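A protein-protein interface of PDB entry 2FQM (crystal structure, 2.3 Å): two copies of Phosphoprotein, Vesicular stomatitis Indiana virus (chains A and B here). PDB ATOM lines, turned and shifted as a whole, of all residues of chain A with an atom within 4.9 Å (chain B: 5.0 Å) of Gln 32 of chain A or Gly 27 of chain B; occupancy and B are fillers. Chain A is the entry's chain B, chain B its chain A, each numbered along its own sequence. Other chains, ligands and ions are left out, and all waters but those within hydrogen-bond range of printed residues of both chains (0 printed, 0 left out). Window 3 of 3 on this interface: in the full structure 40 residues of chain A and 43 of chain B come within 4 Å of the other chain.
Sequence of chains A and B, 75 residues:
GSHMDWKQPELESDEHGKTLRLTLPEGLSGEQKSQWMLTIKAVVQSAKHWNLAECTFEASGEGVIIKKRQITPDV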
ATOM      1  N   LEU A  28       9.015  33.354  20.063  1.00  0.00           N
ATOM      2  CA  LEU A  28      10.208  32.726  20.639  1.00  0.00           C
ATOM      3  C   LEU A  28      11.324  32.707  19.592  1.00  0.00           C
ATOM      4  O   LEU A  28      11.061  32.806  18.384  1.00  0.00           O
ATOM      5  CB  LEU A  28       9.929  31.277  21.052  1.00  0.00           C
ATOM      6  CG  LEU A  28       9.156  30.951  22.323  1.00  0.00           C
ATOM      7  CD1 LEU A  28       8.974  29.460  22.469  1.00  0.00           C
ATOM      8  CD2 LEU A  28       9.917  31.471  23.463  1.00  0.00           C
ATOM      9  N   SER A  29      12.568  32.586  20.057  1.00  0.00           N
ATOM     10  CA  SER A  29      13.734  32.497  19.162  1.00  0.00           C
ATOM     11  C   SER A  29      13.752  31.112  18.513  1.00  0.00           C
ATOM     12  O   SER A  29      12.878  30.276  18.769  1.00  0.00           O
ATOM     13  CB  SER A  29      15.039  32.679  19.930  1.00  0.00           C
ATOM     14  OG  SER A  29      15.711  31.446  20.108  1.00  0.00           O
ATOM     15  N   GLY A  30      14.756  30.863  17.682  1.00  0.00           N
ATOM     16  CA  GLY A  30      14.854  29.579  16.998  1.00  0.00           C
ATOM     17  C   GLY A  30      15.305  28.438  17.895  1.00  0.00           C
ATOM     18  O   GLY A  30      14.742  27.350  17.820  1.00  0.00           O
ATOM     19  N   GLU A  31      16.288  28.681  18.763  1.00  0.00           N
ATOM     20  CA  GLU A  31      16.781  27.621  19.608  1.00  0.00           C
ATOM     21  C   GLU A  31      15.868  27.459  20.808  1.00  0.00           C
ATOM     22  O   GLU A  31      15.784  26.373  21.380  1.00  0.00           O
ATOM     23  CB  GLU A  31      18.234  27.868  20.050  1.00  0.00           C
ATOM     24  CG  GLU A  31      18.381  28.836  21.199  1.00  0.00           C
ATOM     25  CD  GLU A  31      19.825  29.039  21.622  1.00  0.00           C
ATOM     26  OE1 GLU A  31      20.555  28.023  21.695  1.00  0.00           O
ATOM     27  OE2 GLU A  31      20.226  30.202  21.892  1.00  0.00           O
ATOM     28  N   GLN A  32      15.193  28.525  21.221  1.00  0.00           N
ATOM     29  CA  GLN A  32      14.261  28.366  22.343  1.00  0.00           C
ATOM     30  C   GLN A  32      13.134  27.427  21.865  1.00  0.00           C
ATOM     31  O   GLN A  32      12.687  26.616  22.623  1.00  0.00           O
ATOM     32  CB  GLN A  32      13.668  29.719  22.771  1.00  0.00           C
ATOM     33  CG  GLN A  32      14.585  30.650  23.596  1.00  0.00           C
ATOM     34  CD  GLN A  32      13.913  31.993  23.754  1.00  0.00           C
ATOM     35  OE1 GLN A  32      13.529  32.586  22.749  1.00  0.00           O
ATOM     36  NE2 GLN A  32      13.727  32.473  25.008  1.00  0.00           N
ATOM     37  N   LYS A  33      12.699  27.569  20.610  1.00  0.00           N
ATOM     38  CA  LYS A  33      11.668  26.756  20.009  1.00  0.00           C
ATOM     39  C   LYS A  33      12.104  25.311  19.949  1.00  0.00           C
ATOM     40  O   LYS A  33      11.317  24.429  20.199  1.00  0.00           O
ATOM     41  CB  LYS A  33      11.353  27.221  18.581  1.00  0.00           C
ATOM     42  CG  LYS A  33      10.163  28.137  18.417  1.00  0.00           C
ATOM     43  CD  LYS A  33      10.443  29.233  17.390  1.00  0.00           C
ATOM     44  CE  LYS A  33       9.155  29.813  16.751  1.00  0.00           C
ATOM     45  NZ  LYS A  33       8.522  31.017  17.412  1.00  0.00           N
ATOM     46  N   SER A  34      13.352  25.046  19.605  1.00  0.00           N
ATOM     47  CA  SER A  34      13.780  23.660  19.558  1.00  0.00           C
ATOM     48  C   SER A  34      13.836  23.040  20.963  1.00  0.00           C
ATOM     49  O   SER A  34      13.345  21.940  21.167  1.00  0.00           O
ATOM     50  CB  SER A  34      15.138  23.530  18.854  1.00  0.00           C
ATOM     51  OG  SER A  34      14.978  23.634  17.450  1.00  0.00           O
ATOM     52  N   GLN A  35      14.423  23.745  21.921  1.00  0.00           N
ATOM     53  CA  GLN A  35      14.524  23.271  23.307  1.00  0.00           C
ATOM     54  C   GLN A  35      13.128  22.909  23.824  1.00  0.00           C
ATOM     55  O   GLN A  35      12.914  21.869  24.395  1.00  0.00           O
ATOM     56  CB  GLN A  35      15.118  24.364  24.187  1.00  0.00           C
ATOM     57  CG  GLN A  35      16.486  24.824  23.758  1.00  0.00           C
ATOM     58  CD  GLN A  35      16.963  26.042  24.502  1.00  0.00           C
ATOM     59  OE1 GLN A  35      16.184  26.785  25.111  1.00  0.00           O
ATOM     60  NE2 GLN A  35      18.250  26.269  24.444  1.00  0.00           N
ATOM     61  N   TRP A  36      12.175  23.779  23.546  1.00  0.00           N
ATOM     62  CA  TRP A  36      10.818  23.595  23.984  1.00  0.00           C
ATOM     63  C   TRP A  36      10.264  22.314  23.392  1.00  0.00           C
ATOM     64  O   TRP A  36       9.718  21.487  24.084  1.00  0.00           O
ATOM     65  CB  TRP A  36       9.999  24.769  23.497  1.00  0.00           C
ATOM     66  CG  TRP A  36       8.603  24.890  24.073  1.00  0.00           C
ATOM     67  CD1 TRP A  36       7.601  23.969  24.031  1.00  0.00           C
ATOM     68  CD2 TRP A  36       8.065  26.028  24.743  1.00  0.00           C
ATOM     69  NE1 TRP A  36       6.452  24.464  24.642  1.00  0.00           N
ATOM     70  CE2 TRP A  36       6.720  25.722  25.096  1.00  0.00           C
ATOM     71  CE3 TRP A  36       8.584  27.277  25.079  1.00  0.00           C
ATOM     72  CZ2 TRP A  36       5.899  26.612  25.777  1.00  0.00           C
ATOM     73  CZ3 TRP A  36       7.751  28.187  25.765  1.00  0.00           C
ATOM     74  CH2 TRP A  36       6.424  27.839  26.108  1.00  0.00           C
ATOM     75  N   PRO B  25      13.313  25.829  28.686  1.00  0.00           N
ATOM     76  CA  PRO B  25      13.961  26.496  27.557  1.00  0.00           C
ATOM     77  C   PRO B  25      14.547  27.790  28.174  1.00  0.00           C
ATOM     78  O   PRO B  25      13.896  28.417  29.009  1.00  0.00           O
ATOM     79  CB  PRO B  25      12.784  26.824  26.652  1.00  0.00           C
ATOM     80  CG  PRO B  25      11.861  25.624  26.885  1.00  0.00           C
ATOM     81  CD  PRO B  25      11.940  25.407  28.351  1.00  0.00           C
ATOM     82  N   GLU B  26      15.728  28.229  27.760  1.00  0.00           N
ATOM     83  CA  GLU B  26      16.320  29.433  28.366  1.00  0.00           C
ATOM     84  C   GLU B  26      15.867  30.796  27.823  1.00  0.00           C
ATOM     85  O   GLU B  26      15.438  30.894  26.673  1.00  0.00           O
ATOM     86  CB  GLU B  26      17.855  29.361  28.291  1.00  0.00           C
ATOM     87  CG  GLU B  26      18.604  30.574  28.964  1.00  0.00           C
ATOM     88  CD  GLU B  26      18.262  30.800  30.456  1.00  0.00           C
ATOM     89  OE1 GLU B  26      18.636  31.870  30.993  1.00  0.00           O
ATOM     90  OE2 GLU B  26      17.632  29.917  31.085  1.00  0.00           O
ATOM     91  N   GLY B  27      15.961  31.842  28.673  1.00  0.00           N
ATOM     92  CA  GLY B  27      15.632  33.214  28.269  1.00  0.00           C
ATOM     93  C   GLY B  27      14.165  33.432  28.076  1.00  0.00           C
ATOM     94  O   GLY B  27      13.699  34.114  27.155  1.00  0.00           O
ATOM     95  N   LEU B  28      13.425  32.842  28.998  1.00  0.00           N
ATOM     96  CA  LEU B  28      11.975  32.888  28.958  1.00  0.00           C
ATOM     97  C   LEU B  28      11.404  33.871  29.986  1.00  0.00           C
ATOM     98  O   LEU B  28      11.904  33.993  31.113  1.00  0.00           O
ATOM     99  CB  LEU B  28      11.466  31.452  29.209  1.00  0.00           C
ATOM    100  CG  LEU B  28      10.797  30.603  28.110  1.00  0.00           C
ATOM    101  CD1 LEU B  28      11.469  30.735  26.777  1.00  0.00           C
ATOM    102  CD2 LEU B  28      10.762  29.162  28.565  1.00  0.00           C
ATOM    103  N   SER B  29      10.367  34.586  29.592  1.00  0.00           N
ATOM    104  CA  SER B  29       9.694  35.510  30.487  1.00  0.00           C
ATOM    105  C   SER B  29       8.856  34.674  31.459  1.00  0.00           C
ATOM    106  O   SER B  29       8.490  33.556  31.129  1.00  0.00           O
ATOM    107  CB  SER B  29       8.779  36.362  29.668  1.00  0.00           C
ATOM    108  OG  SER B  29       7.816  35.512  29.114  1.00  0.00           O
ATOM    109  N   GLN B  32       5.999  32.947  29.715  1.00  0.00           N
ATOM    110  CA  GLN B  32       6.360  31.793  28.893  1.00  0.00           C
ATOM    111  C   GLN B  32       6.726  30.574  29.740  1.00  0.00           C
ATOM    112  O   GLN B  32       6.408  29.457  29.377  1.00  0.00           O
ATOM    113  CB  GLN B  32       7.528  32.136  27.990  1.00  0.00           C
ATOM    114  CG  GLN B  32       7.298  33.330  27.105  1.00  0.00           C
ATOM    115  CD  GLN B  32       8.617  33.922  26.683  1.00  0.00           C
ATOM    116  OE1 GLN B  32       9.540  34.094  27.494  1.00  0.00           O
ATOM    117  NE2 GLN B  32       8.725  34.236  25.423  1.00  0.00           N
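Hydrophobic or aromatic side chains of chain A within 4 Å of the printed part of chain B: Leu 28 and Trp 36. Hydrophobic or aromatic side chains of chain B that line the printed part of chain A: Pro 25 and Leu 28. Among the printed residues, 9 pairs touch across the chains. Among the printed residues, no Asp or Glu carboxylate lies within 4 Å of a Lys or Arg side-chain nitrogen of the other chain.
The backbone NH of Glu 26 of chain B lies within hydrogen-bond range of the side-chain amide oxygen of Gln 35 of chain A (3.1 Å). The backbone carbonyl oxygen of Glu 26 of chain B lies within hydrogen-bond range of the side-chain amide nitrogen of Gln 32 of chain A, at 2.9 Å. The side-chain amide nitrogen (NE2) of Gln 32 of chain A sits at hydrogen-bond distance from the backbone carbonyl oxygen (O) of Gly 27 of chain B (2.7 Å).
Leu 28 of chain A touches its own counterpart, Leu 28 of chain B. Leu 28 of chain A touches Gln 32 of chain B, and with the chains exchanged Gln 32 of chain A touches Leu 28 of chain B.
Of the printed residues of chain B, Leu 28 of chain A touches Leu 28 and Gln 32. Gly 30 of chain A touches none of the printed residues of chain B. Of the printed residues of chain B, Gln 35 of chain A touches Pro 25 and Glu 26. Of the printed residues of chain B, Trp 36 of chain A touches Pro 25 (3.7 Å) and Gln 32 (3.6 Å). Gly 27 of chain B touches just one residue of chain A: Gln 32. Of the printed residues of chain A, Leu 28 of chain B touches Leu 28 and Gln 32. Of the printed residues of chain A, Gln 32 of chain B touches Leu 28 and Trp 36. The nearest residue of chain B that does not touch Gln 32 of chain A is Pro 25 of chain B (4.04 Å). The nearest printed residue of chain A that does not touch Leu 28 of chain B is Trp 36 of chain A (4.2 Å).
OE1 of Gln 32 of chain B sits at hydrogen-bond distance from OG of Ser 29 of chain B. The backbone NH of Ser 29 of chain A lies within hydrogen-bond range of the side-chain amide oxygen of Gln 32 of chain A (2.9 Å). O of Leu 28 of chain A sits at hydrogen-bond distance from NZ of Lys 33 of chain A (3.3 Å).
CD2 of Leu 28 of chain A touches CD1 of Leu 28 of chain B, at 3.7 Å. CD2 of Leu 28 of chain A touches NE2 of Gln 32 of chain B (3.6 Å). NE2 of Gln 32 of chain A touches CD1 of Leu 28 of chain B, at 3.4 Å. CA of Pro 25 of chain B touches OE1 of Gln 35 of chain A, 3.3 Å away. Trp 36 of chain A touches Pro 25 of chain B. CH2 of Trp 36 of chain A touches O of Gln 32 of chain B (3.6 Å).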
